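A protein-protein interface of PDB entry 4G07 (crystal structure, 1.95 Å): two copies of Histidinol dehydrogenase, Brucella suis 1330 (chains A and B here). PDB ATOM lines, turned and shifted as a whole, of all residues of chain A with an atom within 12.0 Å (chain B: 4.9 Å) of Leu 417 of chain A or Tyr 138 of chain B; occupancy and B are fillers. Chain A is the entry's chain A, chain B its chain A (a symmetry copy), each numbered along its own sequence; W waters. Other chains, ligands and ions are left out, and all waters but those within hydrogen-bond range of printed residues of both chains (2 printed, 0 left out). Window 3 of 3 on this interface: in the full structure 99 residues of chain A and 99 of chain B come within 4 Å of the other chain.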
ATOM      1  N   GLY A 405     -12.518   6.166  -8.806  1.00  0.00           N
ATOM      2  CA  GLY A 405     -12.057   5.555 -10.046  1.00  0.00           C
ATOM      3  C   GLY A 405     -10.849   4.633  -9.933  1.00  0.00           C
ATOM      4  O   GLY A 405     -10.850   3.535 -10.490  1.00  0.00           O
ATOM      5  N   PRO A 406      -9.788   5.053  -9.239  1.00  0.00           N
ATOM      6  CA  PRO A 406      -8.627   4.168  -9.130  1.00  0.00           C
ATOM      7  C   PRO A 406      -8.978   2.773  -8.603  1.00  0.00           C
ATOM      8  O   PRO A 406      -8.509   1.766  -9.140  1.00  0.00           O
ATOM      9  CB  PRO A 406      -7.701   4.944  -8.199  1.00  0.00           C
ATOM     10  CG  PRO A 406      -7.977   6.377  -8.623  1.00  0.00           C
ATOM     11  CD  PRO A 406      -9.496   6.382  -8.671  1.00  0.00           C
ATOM     12  N   ALA A 407      -9.795   2.708  -7.558  1.00  0.00           N
ATOM     13  CA  ALA A 407     -10.184   1.419  -6.993  1.00  0.00           C
ATOM     14  C   ALA A 407     -10.897   0.568  -8.035  1.00  0.00           C
ATOM     15  O   ALA A 407     -10.665  -0.640  -8.137  1.00  0.00           O
ATOM     16  CB  ALA A 407     -11.086   1.614  -5.774  1.00  0.00           C
ATOM     17  N   ALA A 408     -11.770   1.200  -8.809  1.00  0.00           N
ATOM     18  CA  ALA A 408     -12.508   0.495  -9.854  1.00  0.00           C
ATOM     19  C   ALA A 408     -11.552  -0.074 -10.904  1.00  0.00           C
ATOM     20  O   ALA A 408     -11.691  -1.213 -11.334  1.00  0.00           O
ATOM     21  CB  ALA A 408     -13.503   1.453 -10.515  1.00  0.00           C
ATOM     22  N   ILE A 409     -10.583   0.734 -11.319  1.00  0.00           N
ATOM     23  CA  ILE A 409      -9.614   0.310 -12.318  1.00  0.00           C
ATOM     24  C   ILE A 409      -8.831  -0.903 -11.808  1.00  0.00           C
ATOM     25  O   ILE A 409      -8.646  -1.896 -12.526  1.00  0.00           O
ATOM     26  CB  ILE A 409      -8.648   1.484 -12.646  1.00  0.00           C
ATOM     27  CG1 ILE A 409      -9.413   2.585 -13.395  1.00  0.00           C
ATOM     28  CG2 ILE A 409      -7.480   0.985 -13.486  1.00  0.00           C
ATOM     29  CD1 ILE A 409      -8.584   3.812 -13.708  1.00  0.00           C
ATOM     30  N   GLU A 410      -8.382  -0.819 -10.561  1.00  0.00           N
ATOM     31  CA  GLU A 410      -7.617  -1.894  -9.927  1.00  0.00           C
ATOM     32  C   GLU A 410      -8.389  -3.222 -10.003  1.00  0.00           C
ATOM     33  O   GLU A 410      -7.851  -4.248 -10.447  1.00  0.00           O
ATOM     34  CB  GLU A 410      -7.331  -1.515  -8.471  1.00  0.00           C
ATOM     35  CG  GLU A 410      -6.515  -2.515  -7.653  1.00  0.00           C
ATOM     36  CD  GLU A 410      -5.033  -2.612  -8.074  1.00  0.00           C
ATOM     37  OE1 GLU A 410      -4.483  -1.642  -8.640  1.00  0.00           O
ATOM     38  OE2 GLU A 410      -4.418  -3.664  -7.810  1.00  0.00           O
ATOM     39  N   ILE A 411      -9.653  -3.199  -9.581  1.00  0.00           N
ATOM     40  CA  ILE A 411     -10.481  -4.394  -9.617  1.00  0.00           C
ATOM     41  C   ILE A 411     -10.754  -4.872 -11.054  1.00  0.00           C
ATOM     42  O   ILE A 411     -10.666  -6.069 -11.346  1.00  0.00           O
ATOM     43  CB  ILE A 411     -11.840  -4.155  -8.905  1.00  0.00           C
ATOM     44  CG1 ILE A 411     -11.590  -3.747  -7.459  1.00  0.00           C
ATOM     45  CG2 ILE A 411     -12.704  -5.454  -8.941  1.00  0.00           C
ATOM     46  CD1 ILE A 411     -12.846  -3.313  -6.730  1.00  0.00           C
ATOM     47  N   ALA A 412     -11.085  -3.948 -11.949  1.00  0.00           N
ATOM     48  CA  ALA A 412     -11.368  -4.325 -13.337  1.00  0.00           C
ATOM     49  C   ALA A 412     -10.169  -5.022 -13.976  1.00  0.00           C
ATOM     50  O   ALA A 412     -10.313  -6.031 -14.677  1.00  0.00           O
ATOM     51  CB  ALA A 412     -11.741  -3.096 -14.155  1.00  0.00           C
ATOM     52  N   ARG A 413      -8.986  -4.468 -13.745  1.00  0.00           N
ATOM     53  CA  ARG A 413      -7.791  -5.068 -14.305  1.00  0.00           C
ATOM     54  C   ARG A 413      -7.487  -6.403 -13.636  1.00  0.00           C
ATOM     55  O   ARG A 413      -7.038  -7.321 -14.300  1.00  0.00           O
ATOM     56  CB  ARG A 413      -6.611  -4.106 -14.210  1.00  0.00           C
ATOM     57  CG  ARG A 413      -6.602  -3.147 -15.398  1.00  0.00           C
ATOM     58  CD  ARG A 413      -5.581  -2.050 -15.264  1.00  0.00           C
ATOM     59  NE  ARG A 413      -5.770  -1.044 -16.299  1.00  0.00           N
ATOM     60  CZ  ARG A 413      -5.306   0.200 -16.229  1.00  0.00           C
ATOM     61  NH1 ARG A 413      -4.611   0.602 -15.162  1.00  0.00           N
ATOM     62  NH2 ARG A 413      -5.554   1.052 -17.220  1.00  0.00           N
ATOM     63  N   ALA A 414      -7.745  -6.516 -12.338  1.00  0.00           N
ATOM     64  CA  ALA A 414      -7.511  -7.780 -11.653  1.00  0.00           C
ATOM     65  C   ALA A 414      -8.490  -8.833 -12.198  1.00  0.00           C
ATOM     66  O   ALA A 414      -8.240 -10.031 -12.097  1.00  0.00           O
ATOM     67  CB  ALA A 414      -7.688  -7.603 -10.152  1.00  0.00           C
ATOM     68  N   GLU A 415      -9.602  -8.388 -12.781  1.00  0.00           N
ATOM     69  CA  GLU A 415     -10.593  -9.307 -13.356  1.00  0.00           C
ATOM     70  C   GLU A 415     -10.410  -9.531 -14.869  1.00  0.00           C
ATOM     71  O   GLU A 415     -11.168 -10.278 -15.489  1.00  0.00           O
ATOM     72  CB  GLU A 415     -12.019  -8.795 -13.109  1.00  0.00           C
ATOM     73  CG  GLU A 415     -12.359  -8.565 -11.648  1.00  0.00           C
ATOM     74  CD  GLU A 415     -13.834  -8.271 -11.433  1.00  0.00           C
ATOM     75  OE1 GLU A 415     -14.444  -7.622 -12.314  1.00  0.00           O
ATOM     76  OE2 GLU A 415     -14.378  -8.682 -10.385  1.00  0.00           O
ATOM     77  N   GLY A 416      -9.412  -8.882 -15.453  1.00  0.00           N
ATOM     78  CA  GLY A 416      -9.149  -9.030 -16.876  1.00  0.00           C
ATOM     79  C   GLY A 416     -10.144  -8.267 -17.733  1.00  0.00           C
ATOM     80  O   GLY A 416     -10.292  -8.531 -18.923  1.00  0.00           O
ATOM     81  N   LEU A 417     -10.831  -7.308 -17.129  1.00  0.00           N
ATOM     82  CA  LEU A 417     -11.827  -6.532 -17.858  1.00  0.00           C
ATOM     83  C   LEU A 417     -11.233  -5.176 -18.220  1.00  0.00           C
ATOM     84  O   LEU A 417     -11.509  -4.166 -17.582  1.00  0.00           O
ATOM     85  CB  LEU A 417     -13.088  -6.381 -16.997  1.00  0.00           C
ATOM     86  CG  LEU A 417     -13.826  -7.695 -16.682  1.00  0.00           C
ATOM     87  CD1 LEU A 417     -14.933  -7.459 -15.670  1.00  0.00           C
ATOM     88  CD2 LEU A 417     -14.408  -8.267 -17.958  1.00  0.00           C
ATOM     89  N   ASP A 418     -10.408  -5.178 -19.259  1.00  0.00           N
ATOM     90  CA  ASP A 418      -9.715  -3.981 -19.713  1.00  0.00           C
ATOM     91  C   ASP A 418     -10.591  -2.867 -20.251  1.00  0.00           C
ATOM     92  O   ASP A 418     -10.299  -1.703 -20.021  1.00  0.00           O
ATOM     93  CB  ASP A 418      -8.666  -4.373 -20.750  1.00  0.00           C
ATOM     94  CG  ASP A 418      -7.614  -5.286 -20.168  1.00  0.00           C
ATOM     95  OD1 ASP A 418      -6.953  -4.866 -19.182  1.00  0.00           O
ATOM     96  OD2 ASP A 418      -7.459  -6.416 -20.689  1.00  0.00           O
ATOM     97  N   ALA A 419     -11.644  -3.214 -20.983  1.00  0.00           N
ATOM     98  CA  ALA A 419     -12.554  -2.190 -21.497  1.00  0.00           C
ATOM     99  C   ALA A 419     -13.206  -1.487 -20.297  1.00  0.00           C
ATOM    100  O   ALA A 419     -13.386  -0.265 -20.301  1.00  0.00           O
ATOM    101  CB  ALA A 419     -13.620  -2.827 -22.395  1.00  0.00           C
ATOM    102  N   HIS A 420     -13.548  -2.257 -19.259  1.00  0.00           N
ATOM    103  CA  HIS A 420     -14.151  -1.681 -18.071  1.00  0.00           C
ATOM    104  C   HIS A 420     -13.172  -0.726 -17.422  1.00  0.00           C
ATOM    105  O   HIS A 420     -13.546   0.361 -16.987  1.00  0.00           O
ATOM    106  CB  HIS A 420     -14.518  -2.757 -17.047  1.00  0.00           C
ATOM    107  CG  HIS A 420     -15.821  -3.438 -17.320  1.00  0.00           C
ATOM    108  ND1 HIS A 420     -16.023  -4.259 -18.408  1.00  0.00           N
ATOM    109  CD2 HIS A 420     -16.973  -3.463 -16.611  1.00  0.00           C
ATOM    110  CE1 HIS A 420     -17.241  -4.768 -18.354  1.00  0.00           C
ATOM    111  NE2 HIS A 420     -17.838  -4.300 -17.273  1.00  0.00           N
ATOM    112  N   ALA A 421     -11.914  -1.138 -17.341  1.00  0.00           N
ATOM    113  CA  ALA A 421     -10.896  -0.279 -16.739  1.00  0.00           C
ATOM    114  C   ALA A 421     -10.706   0.982 -17.578  1.00  0.00           C
ATOM    115  O   ALA A 421     -10.575   2.084 -17.036  1.00  0.00           O
ATOM    116  CB  ALA A 421      -9.573  -1.040 -16.623  1.00  0.00           C
ATOM    117  N   GLN A 422     -10.702   0.823 -18.897  1.00  0.00           N
ATOM    118  CA  GLN A 422     -10.515   1.969 -19.784  1.00  0.00           C
ATOM    119  C   GLN A 422     -11.617   3.034 -19.731  1.00  0.00           C
ATOM    120  O   GLN A 422     -11.328   4.223 -19.871  1.00  0.00           O
ATOM    121  CB  GLN A 422     -10.333   1.501 -21.226  1.00  0.00           C
ATOM    122  CG  GLN A 422      -8.892   1.131 -21.538  1.00  0.00           C
ATOM    123  CD  GLN A 422      -7.918   2.215 -21.091  1.00  0.00           C
ATOM    124  OE1 GLN A 422      -7.987   3.359 -21.555  1.00  0.00           O
ATOM    125  NE2 GLN A 422      -7.019   1.863 -20.176  1.00  0.00           N
ATOM    126  N   SER A 423     -12.867   2.628 -19.529  1.00  0.00           N
ATOM    127  CA  SER A 423     -13.947   3.613 -19.462  1.00  0.00           C
ATOM    128  C   SER A 423     -13.735   4.559 -18.265  1.00  0.00           C
ATOM    129  O   SER A 423     -14.254   5.683 -18.248  1.00  0.00           O
ATOM    130  CB  SER A 423     -15.320   2.917 -19.382  1.00  0.00           C
ATOM    131  OG  SER A 423     -15.475   2.234 -18.154  1.00  0.00           O
ATOM    132  N   VAL A 424     -12.975   4.113 -17.261  1.00  0.00           N
ATOM    133  CA  VAL A 424     -12.678   4.974 -16.117  1.00  0.00           C
ATOM    134  C   VAL A 424     -11.370   5.721 -16.410  1.00  0.00           C
ATOM    135  O   VAL A 424     -11.283   6.940 -16.247  1.00  0.00           O
ATOM    136  CB  VAL A 424     -12.502   4.174 -14.799  1.00  0.00           C
ATOM    137  CG1 VAL A 424     -12.151   5.135 -13.660  1.00  0.00           C
ATOM    138  CG2 VAL A 424     -13.787   3.423 -14.456  1.00  0.00           C
ATOM    139  N   ALA A 425     -10.359   4.983 -16.859  1.00  0.00           N
ATOM    140  CA  ALA A 425      -9.061   5.578 -17.159  1.00  0.00           C
ATOM    141  C   ALA A 425      -9.131   6.715 -18.195  1.00  0.00           C
ATOM    142  O   ALA A 425      -8.438   7.724 -18.053  1.00  0.00           O
ATOM    143  CB  ALA A 425      -8.079   4.485 -17.634  1.00  0.00           C
ATOM    144  N   ILE A 426      -9.970   6.570 -19.222  1.00  0.00           N
ATOM    145  CA  ILE A 426     -10.067   7.596 -20.262  1.00  0.00           C
ATOM    146  C   ILE A 426     -10.548   8.926 -19.686  1.00  0.00           C
ATOM    147  O   ILE A 426     -10.224   9.998 -20.207  1.00  0.00           O
ATOM    148  CB  ILE A 426     -10.993   7.139 -21.426  1.00  0.00           C
ATOM    149  CG1 ILE A 426     -10.771   8.027 -22.655  1.00  0.00           C
ATOM    150  CG2 ILE A 426     -12.457   7.249 -21.033  1.00  0.00           C
ATOM    151  CD1 ILE A 426     -11.357   7.442 -23.909  1.00  0.00           C
ATOM    152  N   VAL B 131     -21.426 -18.899  -7.988  1.00  0.00           N
ATOM    153  CA  VAL B 131     -20.387 -18.097  -8.640  1.00  0.00           C
ATOM    154  C   VAL B 131     -19.700 -18.948  -9.723  1.00  0.00           C
ATOM    155  O   VAL B 131     -19.128 -19.988  -9.428  1.00  0.00           O
ATOM    156  CB  VAL B 131     -19.323 -17.646  -7.611  1.00  0.00           C
ATOM    157  CG1 VAL B 131     -18.211 -16.865  -8.306  1.00  0.00           C
ATOM    158  CG2 VAL B 131     -19.976 -16.788  -6.517  1.00  0.00           C
ATOM    159  N   THR B 135     -12.450 -18.363 -15.908  1.00  0.00           N
ATOM    160  CA  THR B 135     -12.286 -16.972 -16.327  1.00  0.00           C
ATOM    161  C   THR B 135     -13.510 -16.081 -16.114  1.00  0.00           C
ATOM    162  O   THR B 135     -13.431 -14.854 -16.267  1.00  0.00           O
ATOM    163  CB  THR B 135     -11.880 -16.920 -17.807  1.00  0.00           C
ATOM    164  OG1 THR B 135     -12.802 -17.706 -18.576  1.00  0.00           O
ATOM    165  CG2 THR B 135     -10.463 -17.476 -17.986  1.00  0.00           C
ATOM    166  N   ALA B 136     -14.639 -16.691 -15.766  1.00  0.00           N
ATOM    167  CA  ALA B 136     -15.860 -15.935 -15.529  1.00  0.00           C
ATOM    168  C   ALA B 136     -16.048 -15.716 -14.028  1.00  0.00           C
ATOM    169  O   ALA B 136     -17.051 -15.146 -13.602  1.00  0.00           O
ATOM    170  CB  ALA B 136     -17.061 -16.685 -16.106  1.00  0.00           C
ATOM    171  N   SER B 137     -15.060 -16.152 -13.246  1.00  0.00           N
ATOM    172  CA  SER B 137     -15.086 -16.064 -11.783  1.00  0.00           C
ATOM    173  C   SER B 137     -14.590 -14.700 -11.266  1.00  0.00           C
ATOM    174  O   SER B 137     -13.377 -14.485 -11.106  1.00  0.00           O
ATOM    175  CB  SER B 137     -14.231 -17.208 -11.215  1.00  0.00           C
ATOM    176  OG  SER B 137     -14.531 -17.477  -9.858  1.00  0.00           O
ATOM    177  N   TYR B 138     -15.531 -13.797 -10.974  1.00  0.00           N
ATOM    178  CA  TYR B 138     -15.186 -12.442 -10.526  1.00  0.00           C
ATOM    179  C   TYR B 138     -15.397 -12.116  -9.057  1.00  0.00           C
ATOM    180  O   TYR B 138     -16.473 -12.341  -8.503  1.00  0.00           O
ATOM    181  CB  TYR B 138     -15.971 -11.396 -11.329  1.00  0.00           C
ATOM    182  CG  TYR B 138     -15.858 -11.518 -12.828  1.00  0.00           C
ATOM    183  CD1 TYR B 138     -16.974 -11.828 -13.602  1.00  0.00           C
ATOM    184  CD2 TYR B 138     -14.636 -11.333 -13.474  1.00  0.00           C
ATOM    185  CE1 TYR B 138     -16.881 -11.957 -14.984  1.00  0.00           C
ATOM    186  CE2 TYR B 138     -14.530 -11.460 -14.862  1.00  0.00           C
ATOM    187  CZ  TYR B 138     -15.659 -11.774 -15.608  1.00  0.00           C
ATOM    188  OH  TYR B 138     -15.568 -11.929 -16.972  1.00  0.00           O
ATOM    189  N   PRO B 139     -14.376 -11.534  -8.412  1.00  0.00           N
ATOM    190  CA  PRO B 139     -14.487 -11.173  -6.998  1.00  0.00           C
ATOM    191  C   PRO B 139     -15.548 -10.078  -6.774  1.00  0.00           C
ATOM    192  O   PRO B 139     -16.184 -10.050  -5.727  1.00  0.00           O
ATOM    193  CB  PRO B 139     -13.071 -10.704  -6.647  1.00  0.00           C
ATOM    194  CG  PRO B 139     -12.558 -10.183  -7.986  1.00  0.00           C
ATOM    195  CD  PRO B 139     -13.028 -11.241  -8.934  1.00  0.00           C
ATOM    196  N   SER B 140     -15.738  -9.181  -7.743  1.00  0.00           N
ATOM    197  CA  SER B 140     -16.749  -8.117  -7.580  1.00  0.00           C
ATOM    198  C   SER B 140     -18.144  -8.734  -7.501  1.00  0.00           C
ATOM    199  O   SER B 140     -19.015  -8.234  -6.791  1.00  0.00           O
ATOM    200  CB  SER B 140     -16.692  -7.104  -8.734  1.00  0.00           C
ATOM    201  OG  SER B 140     -16.909  -7.713  -9.998  1.00  0.00           O
ATOM    202  N   SER B 141     -18.347  -9.823  -8.233  1.00  0.00           N
ATOM    203  CA  SER B 141     -19.629 -10.520  -8.220  1.00  0.00           C
ATOM    204  C   SER B 141     -19.893 -11.076  -6.823  1.00  0.00           C
ATOM    205  O   SER B 141     -21.021 -11.032  -6.324  1.00  0.00           O
ATOM    206  CB  SER B 141     -19.617 -11.674  -9.226  1.00  0.00           C
ATOM    207  OG  SER B 141     -19.434 -11.196 -10.553  1.00  0.00           O
ATOM    208  N   VAL B 142     -18.851 -11.610  -6.201  1.00  0.00           N
ATOM    209  CA  VAL B 142     -18.956 -12.176  -4.861  1.00  0.00           C
ATOM    210  C   VAL B 142     -19.363 -11.113  -3.836  1.00  0.00           C
ATOM    211  O   VAL B 142     -20.253 -11.333  -3.002  1.00  0.00           O
ATOM    212  CB  VAL B 142     -17.608 -12.824  -4.452  1.00  0.00           C
ATOM    213  CG1 VAL B 142     -17.659 -13.336  -3.023  1.00  0.00           C
ATOM    214  CG2 VAL B 142     -17.284 -13.945  -5.434  1.00  0.00           C
ATOM    215  N   VAL B 172     -11.517 -14.658  -5.656  1.00  0.00           N
ATOM    216  CA  VAL B 172     -12.894 -15.006  -5.319  1.00  0.00           C
ATOM    217  C   VAL B 172     -12.926 -15.415  -3.842  1.00  0.00           C
ATOM    218  O   VAL B 172     -13.841 -15.037  -3.109  1.00  0.00           O
ATOM    219  CB  VAL B 172     -13.413 -16.128  -6.228  1.00  0.00           C
ATOM    220  CG1 VAL B 172     -14.637 -16.817  -5.609  1.00  0.00           C
ATOM    221  CG2 VAL B 172     -13.771 -15.522  -7.593  1.00  0.00           C
ATOM    222  N   GLU B 261     -17.392  -6.145 -23.751  1.00  0.00           N
ATOM    223  CA  GLU B 261     -16.397  -7.159 -23.369  1.00  0.00           C
ATOM    224  C   GLU B 261     -16.979  -8.146 -22.362  1.00  0.00           C
ATOM    225  O   GLU B 261     -16.499  -9.276 -22.217  1.00  0.00           O
ATOM    226  CB  GLU B 261     -15.135  -6.518 -22.776  1.00  0.00           C
ATOM    227  CG  GLU B 261     -15.240  -6.088 -21.326  1.00  0.00           C
ATOM    228  CD  GLU B 261     -13.930  -5.510 -20.795  1.00  0.00           C
ATOM    229  OE1 GLU B 261     -13.952  -4.810 -19.760  1.00  0.00           O
ATOM    230  OE2 GLU B 261     -12.876  -5.758 -21.417  1.00  0.00           O
ATOM    231  N   TYR B 362     -18.501  -1.832  -9.414  1.00  0.00           N
ATOM    232  CA  TYR B 362     -17.529  -1.964  -8.336  1.00  0.00           C
ATOM    233  C   TYR B 362     -17.586  -1.141  -7.064  1.00  0.00           C
ATOM    234  O   TYR B 362     -17.654  -1.682  -5.970  1.00  0.00           O
ATOM    235  CB  TYR B 362     -16.127  -1.766  -8.912  1.00  0.00           C
ATOM    236  CG  TYR B 362     -15.783  -2.672 -10.071  1.00  0.00           C
ATOM    237  CD1 TYR B 362     -15.463  -2.144 -11.320  1.00  0.00           C
ATOM    238  CD2 TYR B 362     -15.743  -4.054  -9.912  1.00  0.00           C
ATOM    239  CE1 TYR B 362     -15.109  -2.972 -12.376  1.00  0.00           C
ATOM    240  CE2 TYR B 362     -15.389  -4.887 -10.968  1.00  0.00           C
ATOM    241  CZ  TYR B 362     -15.071  -4.341 -12.188  1.00  0.00           C
ATOM    242  OH  TYR B 362     -14.696  -5.169 -13.222  1.00  0.00           O
HETATM  243  O   HOH W   1     -12.560 -11.679 -18.015  1.00  0.00           O
HETATM  244  O   HOH W   2     -17.252  -7.651 -13.349  1.00  0.00           O
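The side-chain hydroxyl of Ser 140 of chain B lies within hydrogen-bond range of the side-chain carboxylate of Glu 415 of chain A (2.7 Å).
OE1 of Glu 415 of chain A sits at hydrogen-bond distance from OH of Tyr 362 of chain B, at 2.6 Å.
OE2 of Glu 261 of chain B lies within hydrogen-bond range of N of Asp 418 of chain A (3.3 Å).
The side-chain carboxylate (OE2) of Glu 261 of chain B is in hydrogen-bond range of the backbone NH (N) of Ala 419 of chain A (2.9 Å).
A ring nitrogen (ND1) of His 420 of chain A is in hydrogen-bond range of the side-chain carboxylate of Glu 261 of chain B (2.5 Å).
The side-chain carboxylate of Glu 415 of chain A lies close to the backbone nitrogen of Pro 139 of chain B.
The backbone carbonyl oxygen (O) of Leu 417 of chain A sits close to the side-chain carboxylate (OE1) of Glu 261 of chain B, 3.3 Å away.
Hydrophobic or aromatic side chains of chain B that line the printed part of chain A: Tyr 138, Pro 139 and Tyr 362.
Hydrophobic or aromatic side chains of chain A that line the printed part of chain B: Ile 411, Ala 412, Leu 417, Ala 419 and His 420.
Water W2 bridges the side-chain carboxylate of Glu 415 of chain A (3.0 Å) and the side-chain hydroxyl of Ser 140 of chain B (3.4 Å).
Water W1 lies within hydrogen-bond range of the side-chain hydroxyl of Tyr 138 of chain B (3.2 Å) and the backbone carbonyl oxygen of Glu 415 of chain A (3.2 Å).
Among the printed residues, pairs that only touch across the chains: Ala 408 of chain A with Tyr 362 of chain B (3.9 Å), Ile 411 of chain A with Tyr 362 of chain B (3.4 Å), Ala 412 of chain A with Tyr 362 of chain B (3.4 Å), Glu 415 of chain A with Tyr 138 of chain B (3.3 Å), Leu 417 of chain A with Tyr 138 of chain B (3.97 Å) and Leu 417 of chain A with Tyr 362 of chain B (3.4 Å).
Leu 417 of chain A touches just these residues of chain B: Tyr 138, Glu 261 and Tyr 362.
Of chain A, only Glu 415 and Leu 417 come within 4 Å of Tyr 138 of chain B.
No residue of chain A comes within 4 Å of Ser 137 of chain B.
Pro 139 of chain B touches just one residue of chain A: Glu 415.
Ser 140 of chain B touches just one residue of chain A: Glu 415 (2.7 Å).
No residue of chain A comes within 4 Å of Ser 141 of chain B.
No residue of chain A comes within 4 Å of Val 142 of chain B.
No residue of chain A comes within 4 Å of Val 172 of chain B.
Of the printed residues of chain B, Asp 418 of chain A touches Glu 261 (3.3 Å).
Of the printed residues of chain B, Ile 411 of chain A touches Tyr 362.
Printed residues of chain B within 4 Å of Ala 412 of chain A: Tyr 362 (3.4 Å).
Printed residues of chain B within 4 Å of Ala 408 of chain A: Tyr 362 (3.9 Å).
Arg 413 of chain A touches none of the printed residues of chain B.
Ala 425 of chain A touches none of the printed residues of chain B.
The nearest printed residue of chain B that does not touch Leu 417 of chain A is Ser 140 of chain B (6.0 Å).
The nearest printed residue of chain B that does not touch Glu 415 of chain A is Ser 141 of chain B (4.7 Å).
No position is printed for both chains.
O of Ala 412 of chain A lies within hydrogen-bond range of N of Leu 417 of chain A, 2.8 Å away.
O of His 420 of chain A sits at hydrogen-bond distance from OG of Ser 423 of chain A (2.9 Å).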
